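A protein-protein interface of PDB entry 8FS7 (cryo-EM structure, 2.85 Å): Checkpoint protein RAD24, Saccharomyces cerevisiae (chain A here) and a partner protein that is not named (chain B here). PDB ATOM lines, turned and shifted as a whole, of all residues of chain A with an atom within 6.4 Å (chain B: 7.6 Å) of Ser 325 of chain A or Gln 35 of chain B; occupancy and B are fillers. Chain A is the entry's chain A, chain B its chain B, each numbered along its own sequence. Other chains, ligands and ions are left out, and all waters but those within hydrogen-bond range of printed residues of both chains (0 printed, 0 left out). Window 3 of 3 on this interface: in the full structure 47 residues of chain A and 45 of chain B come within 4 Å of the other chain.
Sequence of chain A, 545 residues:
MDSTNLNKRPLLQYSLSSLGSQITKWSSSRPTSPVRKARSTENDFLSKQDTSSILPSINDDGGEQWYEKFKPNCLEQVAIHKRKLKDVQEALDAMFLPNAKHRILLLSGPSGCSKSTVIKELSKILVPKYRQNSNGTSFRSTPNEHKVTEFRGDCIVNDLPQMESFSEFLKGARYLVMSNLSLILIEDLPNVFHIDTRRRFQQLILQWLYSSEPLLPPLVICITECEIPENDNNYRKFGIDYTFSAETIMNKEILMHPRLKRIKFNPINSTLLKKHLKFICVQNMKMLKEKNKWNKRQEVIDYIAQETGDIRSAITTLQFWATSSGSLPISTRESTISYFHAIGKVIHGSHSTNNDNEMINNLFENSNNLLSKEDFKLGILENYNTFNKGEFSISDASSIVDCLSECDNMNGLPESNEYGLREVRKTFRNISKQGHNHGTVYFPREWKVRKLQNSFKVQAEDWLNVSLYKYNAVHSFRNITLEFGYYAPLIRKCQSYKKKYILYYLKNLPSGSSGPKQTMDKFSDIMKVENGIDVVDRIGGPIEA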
ATOM      1  N   LYS A 291       8.681  -3.222  24.868  1.00  0.00           N
ATOM      2  CA  LYS A 291       7.915  -4.268  24.202  1.00  0.00           C
ATOM      3  C   LYS A 291       6.805  -4.834  25.078  1.00  0.00           C
ATOM      4  O   LYS A 291       6.281  -5.905  24.763  1.00  0.00           O
ATOM      5  CB  LYS A 291       8.844  -5.401  23.754  1.00  0.00           C
ATOM      6  CG  LYS A 291       9.502  -5.184  22.398  1.00  0.00           C
ATOM      7  CD  LYS A 291      10.727  -4.289  22.502  1.00  0.00           C
ATOM      8  CE  LYS A 291      11.528  -4.297  21.211  1.00  0.00           C
ATOM      9  NZ  LYS A 291      12.017  -5.661  20.869  1.00  0.00           N
ATOM     10  N   LYS A 293       6.705  -6.561  27.542  1.00  0.00           N
ATOM     11  CA  LYS A 293       6.939  -7.916  28.015  1.00  0.00           C
ATOM     12  C   LYS A 293       7.411  -7.963  29.463  1.00  0.00           C
ATOM     13  O   LYS A 293       7.686  -9.054  29.973  1.00  0.00           O
ATOM     14  CB  LYS A 293       7.967  -8.616  27.119  1.00  0.00           C
ATOM     15  CG  LYS A 293       7.486  -8.859  25.698  1.00  0.00           C
ATOM     16  CD  LYS A 293       8.318  -9.924  25.006  1.00  0.00           C
ATOM     17  CE  LYS A 293       7.670 -10.369  23.706  1.00  0.00           C
ATOM     18  NZ  LYS A 293       8.373 -11.535  23.105  1.00  0.00           N
ATOM     19  N   PHE A 320      16.103 -14.693  22.905  1.00  0.00           N
ATOM     20  CA  PHE A 320      15.258 -14.916  21.736  1.00  0.00           C
ATOM     21  C   PHE A 320      13.821 -14.487  22.004  1.00  0.00           C
ATOM     22  O   PHE A 320      13.168 -13.896  21.136  1.00  0.00           O
ATOM     23  CB  PHE A 320      15.315 -16.389  21.331  1.00  0.00           C
ATOM     24  CG  PHE A 320      14.941 -16.641  19.898  1.00  0.00           C
ATOM     25  CD1 PHE A 320      15.717 -16.138  18.867  1.00  0.00           C
ATOM     26  CD2 PHE A 320      13.817 -17.387  19.583  1.00  0.00           C
ATOM     27  CE1 PHE A 320      15.376 -16.370  17.548  1.00  0.00           C
ATOM     28  CE2 PHE A 320      13.473 -17.624  18.265  1.00  0.00           C
ATOM     29  CZ  PHE A 320      14.253 -17.115  17.247  1.00  0.00           C
ATOM     30  N   TRP A 321      13.308 -14.784  23.200  1.00  0.00           N
ATOM     31  CA  TRP A 321      11.953 -14.372  23.552  1.00  0.00           C
ATOM     32  C   TRP A 321      11.844 -12.855  23.673  1.00  0.00           C
ATOM     33  O   TRP A 321      10.855 -12.262  23.226  1.00  0.00           O
ATOM     34  CB  TRP A 321      11.522 -15.045  24.856  1.00  0.00           C
ATOM     35  CG  TRP A 321      10.329 -14.404  25.498  1.00  0.00           C
ATOM     36  CD1 TRP A 321       9.020 -14.582  25.156  1.00  0.00           C
ATOM     37  CD2 TRP A 321      10.336 -13.483  26.594  1.00  0.00           C
ATOM     38  NE1 TRP A 321       8.211 -13.829  25.970  1.00  0.00           N
ATOM     39  CE2 TRP A 321       8.994 -13.144  26.862  1.00  0.00           C
ATOM     40  CE3 TRP A 321      11.344 -12.910  27.374  1.00  0.00           C
ATOM     41  CZ2 TRP A 321       8.636 -12.258  27.877  1.00  0.00           C
ATOM     42  CZ3 TRP A 321      10.987 -12.033  28.382  1.00  0.00           C
ATOM     43  CH2 TRP A 321       9.645 -11.715  28.624  1.00  0.00           C
ATOM     44  N   ALA A 322      12.845 -12.212  24.280  1.00  0.00           N
ATOM     45  CA  ALA A 322      12.787 -10.767  24.483  1.00  0.00           C
ATOM     46  C   ALA A 322      12.903 -10.012  23.165  1.00  0.00           C
ATOM     47  O   ALA A 322      12.178  -9.037  22.937  1.00  0.00           O
ATOM     48  CB  ALA A 322      13.884 -10.329  25.451  1.00  0.00           C
ATOM     49  N   THR A 323      13.808 -10.442  22.284  1.00  0.00           N
ATOM     50  CA  THR A 323      13.983  -9.771  21.002  1.00  0.00           C
ATOM     51  C   THR A 323      12.843 -10.044  20.030  1.00  0.00           C
ATOM     52  O   THR A 323      12.755  -9.365  19.002  1.00  0.00           O
ATOM     53  CB  THR A 323      15.310 -10.186  20.364  1.00  0.00           C
ATOM     54  OG1 THR A 323      15.394 -11.616  20.318  1.00  0.00           O
ATOM     55  CG2 THR A 323      16.482  -9.638  21.167  1.00  0.00           C
ATOM     56  N   SER A 324      11.977 -11.009  20.326  1.00  0.00           N
ATOM     57  CA  SER A 324      10.850 -11.313  19.462  1.00  0.00           C
ATOM     58  C   SER A 324       9.761 -10.251  19.608  1.00  0.00           C
ATOM     59  O   SER A 324       9.727  -9.479  20.570  1.00  0.00           O
ATOM     60  CB  SER A 324      10.290 -12.698  19.779  1.00  0.00           C
ATOM     61  OG  SER A 324       9.034 -12.895  19.155  1.00  0.00           O
ATOM     62  N   SER A 325       8.856 -10.221  18.626  1.00  0.00           N
ATOM     63  CA  SER A 325       7.744  -9.278  18.624  1.00  0.00           C
ATOM     64  C   SER A 325       6.407  -9.979  18.409  1.00  0.00           C
ATOM     65  O   SER A 325       5.409  -9.317  18.106  1.00  0.00           O
ATOM     66  CB  SER A 325       7.952  -8.198  17.560  1.00  0.00           C
ATOM     67  OG  SER A 325       6.717  -7.778  17.008  1.00  0.00           O
ATOM     68  N   GLY A 326       6.363 -11.300  18.559  1.00  0.00           N
ATOM     69  CA  GLY A 326       5.137 -12.043  18.350  1.00  0.00           C
ATOM     70  C   GLY A 326       4.859 -13.067  19.430  1.00  0.00           C
ATOM     71  O   GLY A 326       5.407 -12.983  20.533  1.00  0.00           O
ATOM     72  N   SER A 327       4.005 -14.041  19.121  1.00  0.00           N
ATOM     73  CA  SER A 327       3.624 -15.094  20.060  1.00  0.00           C
ATOM     74  C   SER A 327       4.312 -16.416  19.741  1.00  0.00           C
ATOM     75  O   SER A 327       3.709 -17.485  19.864  1.00  0.00           O
ATOM     76  CB  SER A 327       2.108 -15.269  20.071  1.00  0.00           C
ATOM     77  OG  SER A 327       1.464 -14.086  20.514  1.00  0.00           O
ATOM     78  N   LEU B  20      11.169 -14.357   1.968  1.00  0.00           N
ATOM     79  CA  LEU B  20      10.493 -14.982   3.099  1.00  0.00           C
ATOM     80  C   LEU B  20       8.978 -14.829   3.030  1.00  0.00           C
ATOM     81  O   LEU B  20       8.264 -15.570   3.714  1.00  0.00           O
ATOM     82  CB  LEU B  20      11.015 -14.398   4.411  1.00  0.00           C
ATOM     83  CG  LEU B  20      12.386 -14.889   4.880  1.00  0.00           C
ATOM     84  CD1 LEU B  20      12.966 -13.947   5.922  1.00  0.00           C
ATOM     85  CD2 LEU B  20      12.292 -16.303   5.427  1.00  0.00           C
ATOM     86  N   GLU B  28       4.256 -18.183  12.445  1.00  0.00           N
ATOM     87  CA  GLU B  28       4.993 -17.548  13.534  1.00  0.00           C
ATOM     88  C   GLU B  28       6.497 -17.603  13.285  1.00  0.00           C
ATOM     89  O   GLU B  28       7.212 -16.618  13.507  1.00  0.00           O
ATOM     90  CB  GLU B  28       4.638 -18.221  14.860  1.00  0.00           C
ATOM     91  CG  GLU B  28       3.153 -18.195  15.184  1.00  0.00           C
ATOM     92  CD  GLU B  28       2.834 -18.830  16.522  1.00  0.00           C
ATOM     93  OE1 GLU B  28       3.072 -20.047  16.675  1.00  0.00           O
ATOM     94  OE2 GLU B  28       2.342 -18.115  17.419  1.00  0.00           O
ATOM     95  N   THR B  29       6.993 -18.749  12.815  1.00  0.00           N
ATOM     96  CA  THR B  29       8.424 -18.885  12.559  1.00  0.00           C
ATOM     97  C   THR B  29       8.868 -18.001  11.398  1.00  0.00           C
ATOM     98  O   THR B  29       9.948 -17.402  11.447  1.00  0.00           O
ATOM     99  CB  THR B  29       8.773 -20.347  12.288  1.00  0.00           C
ATOM    100  OG1 THR B  29       8.128 -21.181  13.259  1.00  0.00           O
ATOM    101  CG2 THR B  29      10.274 -20.555  12.384  1.00  0.00           C
ATOM    102  N   ILE B  30       8.049 -17.902  10.347  1.00  0.00           N
ATOM    103  CA  ILE B  30       8.389 -17.032   9.221  1.00  0.00           C
ATOM    104  C   ILE B  30       8.369 -15.569   9.650  1.00  0.00           C
ATOM    105  O   ILE B  30       9.214 -14.772   9.225  1.00  0.00           O
ATOM    106  CB  ILE B  30       7.448 -17.297   8.028  1.00  0.00           C
ATOM    107  CG1 ILE B  30       7.619 -18.717   7.464  1.00  0.00           C
ATOM    108  CG2 ILE B  30       7.665 -16.274   6.922  1.00  0.00           C
ATOM    109  CD1 ILE B  30       8.990 -19.351   7.669  1.00  0.00           C
ATOM    110  N   ASP B  31       7.416 -15.193  10.506  1.00  0.00           N
ATOM    111  CA  ASP B  31       7.389 -13.831  11.030  1.00  0.00           C
ATOM    112  C   ASP B  31       8.622 -13.540  11.878  1.00  0.00           C
ATOM    113  O   ASP B  31       9.195 -12.446  11.801  1.00  0.00           O
ATOM    114  CB  ASP B  31       6.111 -13.609  11.839  1.00  0.00           C
ATOM    115  CG  ASP B  31       4.875 -13.542  10.966  1.00  0.00           C
ATOM    116  OD1 ASP B  31       4.998 -13.771   9.744  1.00  0.00           O
ATOM    117  OD2 ASP B  31       3.780 -13.265  11.499  1.00  0.00           O
ATOM    118  N   ARG B  32       9.046 -14.509  12.694  1.00  0.00           N
ATOM    119  CA  ARG B  32      10.267 -14.335  13.476  1.00  0.00           C
ATOM    120  C   ARG B  32      11.488 -14.204  12.574  1.00  0.00           C
ATOM    121  O   ARG B  32      12.391 -13.406  12.849  1.00  0.00           O
ATOM    122  CB  ARG B  32      10.444 -15.499  14.450  1.00  0.00           C
ATOM    123  CG  ARG B  32      11.588 -15.308  15.434  1.00  0.00           C
ATOM    124  CD  ARG B  32      11.273 -14.208  16.433  1.00  0.00           C
ATOM    125  NE  ARG B  32      12.324 -14.057  17.431  1.00  0.00           N
ATOM    126  CZ  ARG B  32      13.290 -13.151  17.370  1.00  0.00           C
ATOM    127  NH1 ARG B  32      13.365 -12.287  16.370  1.00  0.00           N
ATOM    128  NH2 ARG B  32      14.203 -13.108  18.336  1.00  0.00           N
ATOM    129  N   LEU B  33      11.537 -14.987  11.493  1.00  0.00           N
ATOM    130  CA  LEU B  33      12.644 -14.878  10.547  1.00  0.00           C
ATOM    131  C   LEU B  33      12.656 -13.515   9.863  1.00  0.00           C
ATOM    132  O   LEU B  33      13.724 -12.934   9.642  1.00  0.00           O
ATOM    133  CB  LEU B  33      12.568 -15.999   9.511  1.00  0.00           C
ATOM    134  CG  LEU B  33      12.880 -17.413  10.005  1.00  0.00           C
ATOM    135  CD1 LEU B  33      12.976 -18.381   8.837  1.00  0.00           C
ATOM    136  CD2 LEU B  33      14.160 -17.430  10.827  1.00  0.00           C
ATOM    137  N   GLN B  34      11.476 -12.994   9.515  1.00  0.00           N
ATOM    138  CA  GLN B  34      11.396 -11.654   8.938  1.00  0.00           C
ATOM    139  C   GLN B  34      11.862 -10.596   9.930  1.00  0.00           C
ATOM    140  O   GLN B  34      12.553  -9.640   9.554  1.00  0.00           O
ATOM    141  CB  GLN B  34       9.966 -11.364   8.479  1.00  0.00           C
ATOM    142  CG  GLN B  34       9.516 -12.167   7.272  1.00  0.00           C
ATOM    143  CD  GLN B  34       9.690 -11.410   5.970  1.00  0.00           C
ATOM    144  OE1 GLN B  34      10.483 -10.472   5.887  1.00  0.00           O
ATOM    145  NE2 GLN B  34       8.942 -11.808   4.949  1.00  0.00           N
ATOM    146  N   GLN B  35      11.481 -10.746  11.202  1.00  0.00           N
ATOM    147  CA  GLN B  35      11.937  -9.814  12.229  1.00  0.00           C
ATOM    148  C   GLN B  35      13.451  -9.869  12.391  1.00  0.00           C
ATOM    149  O   GLN B  35      14.102  -8.834  12.566  1.00  0.00           O
ATOM    150  CB  GLN B  35      11.244 -10.120  13.558  1.00  0.00           C
ATOM    151  CG  GLN B  35       9.794  -9.674  13.621  1.00  0.00           C
ATOM    152  CD  GLN B  35       9.010 -10.397  14.698  1.00  0.00           C
ATOM    153  OE1 GLN B  35       9.575 -10.857  15.691  1.00  0.00           O
ATOM    154  NE2 GLN B  35       7.699 -10.501  14.509  1.00  0.00           N
ATOM    155  N   ILE B  36      14.025 -11.073  12.336  1.00  0.00           N
ATOM    156  CA  ILE B  36      15.477 -11.220  12.408  1.00  0.00           C
ATOM    157  C   ILE B  36      16.141 -10.561  11.205  1.00  0.00           C
ATOM    158  O   ILE B  36      17.161  -9.872  11.339  1.00  0.00           O
ATOM    159  CB  ILE B  36      15.854 -12.710  12.523  1.00  0.00           C
ATOM    160  CG1 ILE B  36      15.447 -13.261  13.891  1.00  0.00           C
ATOM    161  CG2 ILE B  36      17.340 -12.913  12.285  1.00  0.00           C
ATOM    162  CD1 ILE B  36      15.562 -14.766  14.000  1.00  0.00           C
ATOM    163  N   ALA B  37      15.573 -10.758  10.013  1.00  0.00           N
ATOM    164  CA  ALA B  37      16.141 -10.171   8.804  1.00  0.00           C
ATOM    165  C   ALA B  37      16.103  -8.650   8.842  1.00  0.00           C
ATOM    166  O   ALA B  37      17.067  -7.995   8.428  1.00  0.00           O
ATOM    167  CB  ALA B  37      15.401 -10.687   7.570  1.00  0.00           C
ATOM    168  N   LYS B  38      15.008  -8.068   9.329  1.00  0.00           N
ATOM    169  CA  LYS B  38      14.905  -6.617   9.437  1.00  0.00           C
ATOM    170  C   LYS B  38      15.698  -6.055  10.610  1.00  0.00           C
ATOM    171  O   LYS B  38      16.041  -4.868  10.607  1.00  0.00           O
ATOM    172  CB  LYS B  38      13.436  -6.192   9.552  1.00  0.00           C
ATOM    173  CG  LYS B  38      12.959  -5.887  10.964  1.00  0.00           C
ATOM    174  CD  LYS B  38      11.484  -5.521  10.979  1.00  0.00           C
ATOM    175  CE  LYS B  38      10.800  -6.023  12.239  1.00  0.00           C
ATOM    176  NZ  LYS B  38       9.380  -6.398  11.985  1.00  0.00           N
ATOM    177  N   ASP B  39      16.006  -6.882  11.613  1.00  0.00           N
ATOM    178  CA  ASP B  39      16.804  -6.415  12.743  1.00  0.00           C
ATOM    179  C   ASP B  39      18.291  -6.604  12.473  1.00  0.00           C
ATOM    180  O   ASP B  39      19.100  -5.702  12.723  1.00  0.00           O
ATOM    181  CB  ASP B  39      16.386  -7.153  14.015  1.00  0.00           C
ATOM    182  CG  ASP B  39      16.496  -6.287  15.254  1.00  0.00           C
ATOM    183  OD1 ASP B  39      17.319  -5.346  15.252  1.00  0.00           O
ATOM    184  OD2 ASP B  39      15.761  -6.546  16.230  1.00  0.00           O
ATOM    185  N   GLY B  40      18.671  -7.777  11.964  1.00  0.00           N
ATOM    186  CA  GLY B  40      20.034  -8.081  11.606  1.00  0.00           C
ATOM    187  C   GLY B  40      20.766  -8.962  12.600  1.00  0.00           C
ATOM    188  O   GLY B  40      21.639  -9.738  12.196  1.00  0.00           O
ATOM    189  N   ASN B  41      20.429  -8.865  13.887  1.00  0.00           N
ATOM    190  CA  ASN B  41      21.131  -9.613  14.930  1.00  0.00           C
ATOM    191  C   ASN B  41      20.645 -11.063  14.937  1.00  0.00           C
ATOM    192  O   ASN B  41      19.924 -11.519  15.827  1.00  0.00           O
ATOM    193  CB  ASN B  41      20.938  -8.949  16.286  1.00  0.00           C
ATOM    194  CG  ASN B  41      22.024  -7.940  16.598  1.00  0.00           C
ATOM    195  OD1 ASN B  41      23.079  -8.292  17.125  1.00  0.00           O
ATOM    196  ND2 ASN B  41      21.771  -6.677  16.274  1.00  0.00           N
ATOM    197  N   LEU B  62      16.589 -16.116   4.267  1.00  0.00           N
ATOM    198  CA  LEU B  62      17.042 -15.285   5.375  1.00  0.00           C
ATOM    199  C   LEU B  62      18.438 -14.739   5.114  1.00  0.00           C
ATOM    200  O   LEU B  62      18.700 -13.553   5.343  1.00  0.00           O
ATOM    201  CB  LEU B  62      17.012 -16.088   6.676  1.00  0.00           C
ATOM    202  CG  LEU B  62      17.430 -15.355   7.952  1.00  0.00           C
ATOM    203  CD1 LEU B  62      16.533 -14.156   8.200  1.00  0.00           C
ATOM    204  CD2 LEU B  62      17.406 -16.300   9.144  1.00  0.00           C
ATOM    205  N   LEU B  66      19.417 -10.888   4.519  1.00  0.00           N
ATOM    206  CA  LEU B  66      20.286 -10.366   5.562  1.00  0.00           C
ATOM    207  C   LEU B  66      21.610  -9.831   5.035  1.00  0.00           C
ATOM    208  O   LEU B  66      22.201  -8.957   5.677  1.00  0.00           O
ATOM    209  CB  LEU B  66      20.566 -11.453   6.608  1.00  0.00           C
ATOM    210  CG  LEU B  66      20.865 -10.972   8.027  1.00  0.00           C
ATOM    211  CD1 LEU B  66      19.862  -9.914   8.449  1.00  0.00           C
ATOM    212  CD2 LEU B  66      20.857 -12.140   8.998  1.00  0.00           C
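Among the printed residues, pairs that only touch across the chains: Ser 324 of chain A with Arg 32 of chain B (3.4 Å), Phe 320 of chain A with Ile 36 of chain B (3.9 Å) and Ser 324 of chain A with Gln 35 of chain B (3.97 Å).
The backbone carbonyl oxygen (O) of Phe 320 of chain A is in hydrogen-bond range of the guanidinium group (NH2) of Arg 32 of chain B (3.1 Å).
The guanidinium group (NH2) of Arg 32 of chain B is in hydrogen-bond range of the side-chain hydroxyl (OG1) of Thr 323 of chain A (2.8 Å).
The backbone NH (N) of Ser 325 of chain A sits at hydrogen-bond distance from the side-chain amide oxygen (OE1) of Gln 35 of chain B, 3.1 Å away.
O of Ser 327 of chain A lies close to OE2 of Glu 28 of chain B, 2.9 Å away.
Of the 10 printed residues of chain A, 5 touch a printed residue of chain B.
Printed residues of chain A that touch a printed residue of chain B: Phe 320, Thr 323, Ser 324, Ser 325 and Ser 327.
Hydrophobic or aromatic side chains of chain A that line the printed part of chain B: Phe 320.
Hydrophobic or aromatic side chains of chain B that line the printed part of chain A: Ile 36.
Among the printed residues, no Asp or Glu carboxylate lies within 4 Å of a Lys or Arg side-chain nitrogen of the other chain.
The side-chain hydroxyl (OG1) of Thr 323 of chain A sits at hydrogen-bond distance from the backbone carbonyl oxygen (O) of Phe 320 of chain A, at 3.3 Å.
The side-chain hydroxyl of Ser 324 of chain A lies within hydrogen-bond range of the backbone NH of Gly 326 of chain A.
Ser 325 of chain A touches one residue of chain B.
Of chain A, only Ser 324 (3.97 Å) and Ser 325 (3.1 Å) come within 4 Å of Gln 35 of chain B.
Of the printed residues of chain B, Ser 327 of chain A touches Glu 28 (2.9 Å).
Printed residues of chain A within 4 Å of Ile 36 of chain B: Phe 320 (3.9 Å).
The nearest printed residue of chain A that does not touch Arg 32 of chain B is Ser 325 of chain A (5.2 Å).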
